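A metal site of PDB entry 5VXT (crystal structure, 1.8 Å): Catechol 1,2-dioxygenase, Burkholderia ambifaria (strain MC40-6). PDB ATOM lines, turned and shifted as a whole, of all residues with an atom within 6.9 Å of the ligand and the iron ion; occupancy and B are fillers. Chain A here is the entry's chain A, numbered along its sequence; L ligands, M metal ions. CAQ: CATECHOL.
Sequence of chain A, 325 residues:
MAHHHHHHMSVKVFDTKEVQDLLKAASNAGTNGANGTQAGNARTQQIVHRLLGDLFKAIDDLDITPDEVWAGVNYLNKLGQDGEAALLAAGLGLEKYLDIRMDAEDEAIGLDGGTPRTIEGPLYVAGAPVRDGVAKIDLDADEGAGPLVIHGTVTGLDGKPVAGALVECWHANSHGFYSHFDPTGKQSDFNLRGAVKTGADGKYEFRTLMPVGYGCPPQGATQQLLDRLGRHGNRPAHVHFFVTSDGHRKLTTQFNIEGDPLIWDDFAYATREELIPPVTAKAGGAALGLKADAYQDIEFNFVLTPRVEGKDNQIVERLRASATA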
ATOM      1  N   ALA A  86      -9.678   5.118  22.131  1.00  0.00           N
ATOM      2  CA  ALA A  86     -10.820   5.960  22.496  1.00  0.00           C
ATOM      3  C   ALA A  86     -11.262   5.685  23.920  1.00  0.00           C
ATOM      4  O   ALA A  86     -11.822   6.569  24.586  1.00  0.00           O
ATOM      5  CB  ALA A  86     -11.995   5.732  21.543  1.00  0.00           C
ATOM      6  N   LEU A  87     -11.036   4.469  24.413  1.00  0.00           N
ATOM      7  CA  LEU A  87     -11.332   4.172  25.804  1.00  0.00           C
ATOM      8  C   LEU A  87     -10.402   4.946  26.738  1.00  0.00           C
ATOM      9  O   LEU A  87     -10.843   5.477  27.765  1.00  0.00           O
ATOM     10  CB  LEU A  87     -11.203   2.663  26.031  1.00  0.00           C
ATOM     11  CG  LEU A  87     -11.737   2.100  27.342  1.00  0.00           C
ATOM     12  CD1 LEU A  87     -13.225   2.341  27.442  1.00  0.00           C
ATOM     13  CD2 LEU A  87     -11.442   0.619  27.394  1.00  0.00           C
ATOM     14  N   ALA A  90     -11.344   8.574  26.971  1.00  0.00           N
ATOM     15  CA  ALA A  90     -12.360   8.823  27.986  1.00  0.00           C
ATOM     16  C   ALA A  90     -11.764   8.732  29.386  1.00  0.00           C
ATOM     17  O   ALA A  90     -12.025   9.582  30.237  1.00  0.00           O
ATOM     18  CB  ALA A  90     -13.527   7.850  27.824  1.00  0.00           C
ATOM     19  N   GLY A  91     -10.926   7.705  29.608  1.00  0.00           N
ATOM     20  CA  GLY A  91     -10.379   7.473  30.935  1.00  0.00           C
ATOM     21  C   GLY A  91      -9.458   8.558  31.428  1.00  0.00           C
ATOM     22  O   GLY A  91      -9.338   8.769  32.639  1.00  0.00           O
ATOM     23  N   GLU A  95     -12.008  13.103  26.659  1.00  0.00           N
ATOM     24  CA  GLU A  95     -13.332  13.212  26.081  1.00  0.00           C
ATOM     25  C   GLU A  95     -14.178  14.219  26.856  1.00  0.00           C
ATOM     26  O   GLU A  95     -14.896  15.023  26.252  1.00  0.00           O
ATOM     27  CB  GLU A  95     -14.003  11.840  26.032  1.00  0.00           C
ATOM     28  CG  GLU A  95     -15.307  11.820  25.221  1.00  0.00           C
ATOM     29  CD  GLU A  95     -15.767  10.427  24.868  1.00  0.00           C
ATOM     30  OE1 GLU A  95     -15.236   9.447  25.430  1.00  0.00           O
ATOM     31  OE2 GLU A  95     -16.650  10.300  23.986  1.00  0.00           O
ATOM     32  N   ILE A 119     -20.466  12.884  27.467  1.00  0.00           N
ATOM     33  CA  ILE A 119     -19.631  12.218  26.472  1.00  0.00           C
ATOM     34  C   ILE A 119     -20.406  11.144  25.731  1.00  0.00           C
ATOM     35  O   ILE A 119     -21.313  10.499  26.282  1.00  0.00           O
ATOM     36  CB  ILE A 119     -18.371  11.636  27.128  1.00  0.00           C
ATOM     37  CG1 ILE A 119     -18.712  10.437  28.024  1.00  0.00           C
ATOM     38  CG2 ILE A 119     -17.591  12.735  27.866  1.00  0.00           C
ATOM     39  CD1 ILE A 119     -17.473   9.660  28.514  1.00  0.00           C
ATOM     40  N   GLU A 120     -20.036  10.940  24.466  1.00  0.00           N
ATOM     41  CA  GLU A 120     -20.558   9.850  23.658  1.00  0.00           C
ATOM     42  C   GLU A 120     -20.016   8.503  24.121  1.00  0.00           C
ATOM     43  O   GLU A 120     -20.744   7.502  24.149  1.00  0.00           O
ATOM     44  CB  GLU A 120     -20.200  10.074  22.187  1.00  0.00           C
ATOM     45  CG  GLU A 120     -20.675   8.984  21.219  1.00  0.00           C
ATOM     46  CD  GLU A 120     -20.295   9.276  19.795  1.00  0.00           C
ATOM     47  OE1 GLU A 120     -20.099  10.457  19.476  1.00  0.00           O
ATOM     48  OE2 GLU A 120     -20.174   8.322  18.986  1.00  0.00           O
ATOM     49  N   GLY A 121     -18.733   8.458  24.481  1.00  0.00           N
ATOM     50  CA  GLY A 121     -18.093   7.197  24.748  1.00  0.00           C
ATOM     51  C   GLY A 121     -17.859   6.461  23.430  1.00  0.00           C
ATOM     52  O   GLY A 121     -18.323   6.880  22.367  1.00  0.00           O
ATOM     53  N   PRO A 122     -17.131   5.355  23.483  1.00  0.00           N
ATOM     54  CA  PRO A 122     -16.673   4.679  22.261  1.00  0.00           C
ATOM     55  C   PRO A 122     -17.568   3.560  21.743  1.00  0.00           C
ATOM     56  O   PRO A 122     -17.138   2.836  20.842  1.00  0.00           O
ATOM     57  CB  PRO A 122     -15.307   4.124  22.695  1.00  0.00           C
ATOM     58  CG  PRO A 122     -15.574   3.699  24.123  1.00  0.00           C
ATOM     59  CD  PRO A 122     -16.552   4.733  24.701  1.00  0.00           C
ATOM     60  N   LEU A 123     -18.796   3.375  22.263  1.00  0.00           N
ATOM     61  CA  LEU A 123     -19.533   2.135  21.999  1.00  0.00           C
ATOM     62  C   LEU A 123     -20.846   2.362  21.232  1.00  0.00           C
ATOM     63  O   LEU A 123     -21.707   1.482  21.227  1.00  0.00           O
ATOM     64  CB  LEU A 123     -19.811   1.396  23.306  1.00  0.00           C
ATOM     65  CG  LEU A 123     -18.559   1.108  24.158  1.00  0.00           C
ATOM     66  CD1 LEU A 123     -18.907   0.371  25.425  1.00  0.00           C
ATOM     67  CD2 LEU A 123     -17.515   0.353  23.353  1.00  0.00           C
ATOM     68  N   TRP A 170     -28.484   3.549  23.611  1.00  0.00           N
ATOM     69  CA  TRP A 170     -27.721   2.311  23.755  1.00  0.00           C
ATOM     70  C   TRP A 170     -27.191   2.200  25.186  1.00  0.00           C
ATOM     71  O   TRP A 170     -26.947   3.217  25.839  1.00  0.00           O
ATOM     72  CB  TRP A 170     -26.560   2.227  22.727  1.00  0.00           C
ATOM     73  CG  TRP A 170     -25.444   3.276  22.801  1.00  0.00           C
ATOM     74  CD1 TRP A 170     -24.160   3.085  23.250  1.00  0.00           C
ATOM     75  CD2 TRP A 170     -25.500   4.626  22.325  1.00  0.00           C
ATOM     76  NE1 TRP A 170     -23.428   4.236  23.114  1.00  0.00           N
ATOM     77  CE2 TRP A 170     -24.226   5.206  22.556  1.00  0.00           C
ATOM     78  CE3 TRP A 170     -26.497   5.421  21.742  1.00  0.00           C
ATOM     79  CZ2 TRP A 170     -23.936   6.534  22.227  1.00  0.00           C
ATOM     80  CZ3 TRP A 170     -26.209   6.746  21.422  1.00  0.00           C
ATOM     81  CH2 TRP A 170     -24.949   7.292  21.662  1.00  0.00           C
ATOM     82  N   HIS A 171     -27.052   0.965  25.683  1.00  0.00           N
ATOM     83  CA  HIS A 171     -26.609   0.747  27.052  1.00  0.00           C
ATOM     84  C   HIS A 171     -26.225  -0.719  27.249  1.00  0.00           C
ATOM     85  O   HIS A 171     -26.441  -1.563  26.373  1.00  0.00           O
ATOM     86  CB  HIS A 171     -27.693   1.174  28.066  1.00  0.00           C
ATOM     87  CG  HIS A 171     -28.910   0.300  28.078  1.00  0.00           C
ATOM     88  ND1 HIS A 171     -28.944  -0.925  28.704  1.00  0.00           N
ATOM     89  CD2 HIS A 171     -30.139   0.472  27.531  1.00  0.00           C
ATOM     90  CE1 HIS A 171     -30.134  -1.468  28.548  1.00  0.00           C
ATOM     91  NE2 HIS A 171     -30.878  -0.640  27.847  1.00  0.00           N
ATOM     92  N   ALA A 172     -25.660  -1.008  28.416  1.00  0.00           N
ATOM     93  CA  ALA A 172     -25.109  -2.319  28.731  1.00  0.00           C
ATOM     94  C   ALA A 172     -26.144  -3.253  29.340  1.00  0.00           C
ATOM     95  O   ALA A 172     -27.207  -2.824  29.804  1.00  0.00           O
ATOM     96  CB  ALA A 172     -23.930  -2.188  29.690  1.00  0.00           C
ATOM     97  N   TYR A 178     -21.932  -4.327  26.227  1.00  0.00           N
ATOM     98  CA  TYR A 178     -22.714  -3.806  25.112  1.00  0.00           C
ATOM     99  C   TYR A 178     -22.709  -4.777  23.948  1.00  0.00           C
ATOM    100  O   TYR A 178     -21.708  -5.430  23.673  1.00  0.00           O
ATOM    101  CB  TYR A 178     -22.145  -2.481  24.619  1.00  0.00           C
ATOM    102  CG  TYR A 178     -22.307  -1.319  25.549  1.00  0.00           C
ATOM    103  CD1 TYR A 178     -21.595  -1.250  26.734  1.00  0.00           C
ATOM    104  CD2 TYR A 178     -23.161  -0.272  25.222  1.00  0.00           C
ATOM    105  CE1 TYR A 178     -21.721  -0.181  27.584  1.00  0.00           C
ATOM    106  CE2 TYR A 178     -23.306   0.803  26.058  1.00  0.00           C
ATOM    107  CZ  TYR A 178     -22.591   0.843  27.247  1.00  0.00           C
ATOM    108  OH  TYR A 178     -22.726   1.899  28.080  1.00  0.00           O
ATOM    109  N   TYR A 214     -20.332  -0.151  33.732  1.00  0.00           N
ATOM    110  CA  TYR A 214     -19.303  -0.661  32.841  1.00  0.00           C
ATOM    111  C   TYR A 214     -17.939  -0.705  33.533  1.00  0.00           C
ATOM    112  O   TYR A 214     -17.637   0.104  34.410  1.00  0.00           O
ATOM    113  CB  TYR A 214     -19.236   0.218  31.583  1.00  0.00           C
ATOM    114  CG  TYR A 214     -18.098  -0.047  30.616  1.00  0.00           C
ATOM    115  CD1 TYR A 214     -18.285  -0.886  29.514  1.00  0.00           C
ATOM    116  CD2 TYR A 214     -16.856   0.554  30.792  1.00  0.00           C
ATOM    117  CE1 TYR A 214     -17.240  -1.134  28.625  1.00  0.00           C
ATOM    118  CE2 TYR A 214     -15.804   0.297  29.912  1.00  0.00           C
ATOM    119  CZ  TYR A 214     -16.007  -0.544  28.838  1.00  0.00           C
ATOM    120  OH  TYR A 214     -14.979  -0.800  27.963  1.00  0.00           O
ATOM    121  N   CYS A 216     -13.607  -1.281  32.459  1.00  0.00           N
ATOM    122  CA  CYS A 216     -12.625  -1.479  31.385  1.00  0.00           C
ATOM    123  C   CYS A 216     -12.184  -2.939  31.310  1.00  0.00           C
ATOM    124  O   CYS A 216     -12.149  -3.627  32.337  1.00  0.00           O
ATOM    125  CB  CYS A 216     -11.405  -0.583  31.604  1.00  0.00           C
ATOM    126  SG  CYS A 216     -11.675   1.166  31.268  1.00  0.00           S
ATOM    127  N   ARG A 235     -17.489   2.705  35.422  1.00  0.00           N
ATOM    128  CA  ARG A 235     -18.536   3.704  35.267  1.00  0.00           C
ATOM    129  C   ARG A 235     -19.791   3.281  36.035  1.00  0.00           C
ATOM    130  O   ARG A 235     -20.085   2.083  36.142  1.00  0.00           O
ATOM    131  CB  ARG A 235     -18.924   3.906  33.791  1.00  0.00           C
ATOM    132  CG  ARG A 235     -17.789   4.353  32.838  1.00  0.00           C
ATOM    133  CD  ARG A 235     -18.350   5.247  31.711  1.00  0.00           C
ATOM    134  NE  ARG A 235     -18.989   6.408  32.315  1.00  0.00           N
ATOM    135  CZ  ARG A 235     -20.119   6.967  31.911  1.00  0.00           C
ATOM    136  NH1 ARG A 235     -20.768   6.500  30.846  1.00  0.00           N
ATOM    137  NH2 ARG A 235     -20.618   8.002  32.580  1.00  0.00           N
ATOM    138  N   PRO A 236     -20.539   4.236  36.576  1.00  0.00           N
ATOM    139  CA  PRO A 236     -21.884   3.922  37.073  1.00  0.00           C
ATOM    140  C   PRO A 236     -22.762   3.408  35.946  1.00  0.00           C
ATOM    141  O   PRO A 236     -22.506   3.650  34.764  1.00  0.00           O
ATOM    142  CB  PRO A 236     -22.398   5.266  37.599  1.00  0.00           C
ATOM    143  CG  PRO A 236     -21.655   6.295  36.802  1.00  0.00           C
ATOM    144  CD  PRO A 236     -20.256   5.685  36.620  1.00  0.00           C
ATOM    145  N   HIS A 238     -25.615   3.482  33.362  1.00  0.00           N
ATOM    146  CA  HIS A 238     -26.044   4.654  32.591  1.00  0.00           C
ATOM    147  C   HIS A 238     -26.649   4.226  31.259  1.00  0.00           C
ATOM    148  O   HIS A 238     -26.591   3.065  30.858  1.00  0.00           O
ATOM    149  CB  HIS A 238     -24.858   5.585  32.330  1.00  0.00           C
ATOM    150  CG  HIS A 238     -23.762   4.904  31.570  1.00  0.00           C
ATOM    151  ND1 HIS A 238     -22.868   4.054  32.175  1.00  0.00           N
ATOM    152  CD2 HIS A 238     -23.457   4.897  30.257  1.00  0.00           C
ATOM    153  CE1 HIS A 238     -22.040   3.573  31.272  1.00  0.00           C
ATOM    154  NE2 HIS A 238     -22.368   4.066  30.095  1.00  0.00           N
ATOM    155  N   VAL A 239     -27.234   5.207  30.577  1.00  0.00           N
ATOM    156  CA  VAL A 239     -27.854   4.999  29.270  1.00  0.00           C
ATOM    157  C   VAL A 239     -27.449   6.170  28.394  1.00  0.00           C
ATOM    158  O   VAL A 239     -27.468   7.320  28.844  1.00  0.00           O
ATOM    159  CB  VAL A 239     -29.401   4.906  29.392  1.00  0.00           C
ATOM    160  CG1 VAL A 239     -30.034   4.710  28.020  1.00  0.00           C
ATOM    161  CG2 VAL A 239     -29.817   3.760  30.315  1.00  0.00           C
ATOM    162  N   HIS A 240     -27.078   5.883  27.138  1.00  0.00           N
ATOM    163  CA  HIS A 240     -26.638   6.873  26.178  1.00  0.00           C
ATOM    164  C   HIS A 240     -27.785   7.317  25.278  1.00  0.00           C
ATOM    165  O   HIS A 240     -28.662   6.510  24.937  1.00  0.00           O
ATOM    166  CB  HIS A 240     -25.558   6.311  25.264  1.00  0.00           C
ATOM    167  CG  HIS A 240     -24.278   5.948  25.953  1.00  0.00           C
ATOM    168  ND1 HIS A 240     -23.183   6.792  25.965  1.00  0.00           N
ATOM    169  CD2 HIS A 240     -23.886   4.817  26.576  1.00  0.00           C
ATOM    170  CE1 HIS A 240     -22.181   6.195  26.593  1.00  0.00           C
ATOM    171  NE2 HIS A 240     -22.588   5.000  26.982  1.00  0.00           N
ATOM    172  N   GLN A 254     -26.404  11.475  28.157  1.00  0.00           N
ATOM    173  CA  GLN A 254     -26.642  10.232  28.876  1.00  0.00           C
ATOM    174  C   GLN A 254     -27.466  10.575  30.105  1.00  0.00           C
ATOM    175  O   GLN A 254     -27.586  11.734  30.490  1.00  0.00           O
ATOM    176  CB  GLN A 254     -25.343   9.574  29.382  1.00  0.00           C
ATOM    177  CG  GLN A 254     -24.274   9.277  28.336  1.00  0.00           C
ATOM    178  CD  GLN A 254     -23.059   8.634  28.995  1.00  0.00           C
ATOM    179  OE1 GLN A 254     -23.206   7.949  30.008  1.00  0.00           O
ATOM    180  NE2 GLN A 254     -21.858   8.864  28.448  1.00  0.00           N
ATOM    181  N   ASP A 266     -16.891   8.359  38.565  1.00  0.00           N
ATOM    182  CA  ASP A 266     -16.906   7.840  37.211  1.00  0.00           C
ATOM    183  C   ASP A 266     -15.500   7.958  36.622  1.00  0.00           C
ATOM    184  O   ASP A 266     -14.943   9.064  36.600  1.00  0.00           O
ATOM    185  CB  ASP A 266     -17.917   8.669  36.431  1.00  0.00           C
ATOM    186  CG  ASP A 266     -18.005   8.313  34.974  1.00  0.00           C
ATOM    187  OD1 ASP A 266     -17.571   7.211  34.579  1.00  0.00           O
ATOM    188  OD2 ASP A 266     -18.559   9.145  34.227  1.00  0.00           O
ATOM    189  N   PHE A 267     -14.920   6.845  36.144  1.00  0.00           N
ATOM    190  CA  PHE A 267     -13.571   6.921  35.593  1.00  0.00           C
ATOM    191  C   PHE A 267     -13.502   7.732  34.306  1.00  0.00           C
ATOM    192  O   PHE A 267     -12.391   8.122  33.887  1.00  0.00           O
ATOM    193  CB  PHE A 267     -12.991   5.503  35.352  1.00  0.00           C
ATOM    194  CG  PHE A 267     -13.078   5.032  33.917  1.00  0.00           C
ATOM    195  CD1 PHE A 267     -11.951   5.003  33.109  1.00  0.00           C
ATOM    196  CD2 PHE A 267     -14.285   4.605  33.393  1.00  0.00           C
ATOM    197  CE1 PHE A 267     -12.019   4.583  31.790  1.00  0.00           C
ATOM    198  CE2 PHE A 267     -14.367   4.184  32.069  1.00  0.00           C
ATOM    199  CZ  PHE A 267     -13.227   4.157  31.265  1.00  0.00           C
ATOM    200  N   ALA A 268     -14.641   8.038  33.670  1.00  0.00           N
ATOM    201  CA  ALA A 268     -14.672   8.855  32.466  1.00  0.00           C
ATOM    202  C   ALA A 268     -15.241  10.253  32.704  1.00  0.00           C
ATOM    203  O   ALA A 268     -15.431  11.007  31.741  1.00  0.00           O
ATOM    204  CB  ALA A 268     -15.440   8.136  31.364  1.00  0.00           C
ATOM    205  N   ALA A 270     -17.995  11.741  33.324  1.00  0.00           N
ATOM    206  CA  ALA A 270     -19.121  12.133  32.480  1.00  0.00           C
ATOM    207  C   ALA A 270     -20.400  12.411  33.263  1.00  0.00           C
ATOM    208  O   ALA A 270     -21.405  12.802  32.663  1.00  0.00           O
ATOM    209  CB  ALA A 270     -19.406  11.046  31.444  1.00  0.00           C
HETATM  210  C1  CAQ L   1     -16.217   3.742  28.105  1.00  0.00           C
HETATM  211  C2  CAQ L   1     -17.421   3.061  27.960  1.00  0.00           C
HETATM  212  C3  CAQ L   1     -18.612   3.762  28.050  1.00  0.00           C
HETATM  213  O3  CAQ L   1     -19.816   3.149  27.902  1.00  0.00           O
HETATM  214  C4  CAQ L   1     -18.575   5.213  28.298  1.00  0.00           C
HETATM  215  O4  CAQ L   1     -19.754   5.879  28.392  1.00  0.00           O
HETATM  216  C5  CAQ L   1     -17.363   5.853  28.434  1.00  0.00           C
HETATM  217  C6  CAQ L   1     -16.183   5.120  28.344  1.00  0.00           C
HETATM  218 FE    FE M   1     -21.712   3.570  28.117  1.00  0.00          FE
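The side-chain amide nitrogen (NE2) of Gln 254 sits close to a ring nitrogen (ND1) of His 240, 3.5 Å away.
The guanidinium group of Arg 235 lies within hydrogen-bond range of the side-chain amide oxygen of Gln 254 (3.0 Å).
O of Ile 119 lies within hydrogen-bond range of NE2 of Gln 254, at 2.8 Å.
The backbone carbonyl oxygen (O) of Pro 236 lies within hydrogen-bond range of a ring nitrogen (ND1) of His 238.
OE2 of Glu 95 is in hydrogen-bond range of N of Gly 121, at 2.8 Å.
The guanidinium group (NH1) of Arg 235 lies close to a ring nitrogen (ND1) of His 238, at 3.5 Å.
The backbone NH of His 240 lies within hydrogen-bond range of the backbone carbonyl oxygen of Trp 170, 3.0 Å away.
The guanidinium group of Arg 235 lies within salt-bridge range of the side-chain carboxylate of Asp 266, at 2.8 Å.
Within 4 Å of the iron ion: Tyr 178, His 238 and His 240.
Leu 87 touches the ligand.
CB of Ala 90 touches C6 of the ligand (3.8 Å).
Ile 119 touches the ligand.
Gly 121 touches the ligand (CA to C5, 3.99 Å).
Pro 122 touches the ligand.
CD1 of Leu 123 touches O3 of the ligand (3.8 Å).
CE2 of Tyr 214 touches C2 of the ligand, at 3.8 Å.
Gln 254 touches the ligand.
Hydrophobic or aromatic side chains within 4 Å of the ligand: Leu 87, Ala 90, Ile 119, Pro 122, Leu 123, Tyr 178, Tyr 214 and His 240.
Within 4 Å of the ligand: Leu 87, Ala 90, Ile 119, Gly 121, Pro 122, Leu 123, Tyr 178, Tyr 214, Arg 235, His 238, His 240 and Gln 254.
The nearest printed residue that does not touch the ligand is Ala 268 (4.2 Å).
The iron ion is bound by O3 of the ligand (2.0 Å), OH of Tyr 178 (2.0 Å), NE2 of His 240 (2.0 Å) and NE2 of His 238 (2.1 Å).
The iron ion has four donor atoms within binding distance.
The guanidinium group of Arg 235 lies within hydrogen-bond range of an oxygen (O4) of the ligand (2.7 Å).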
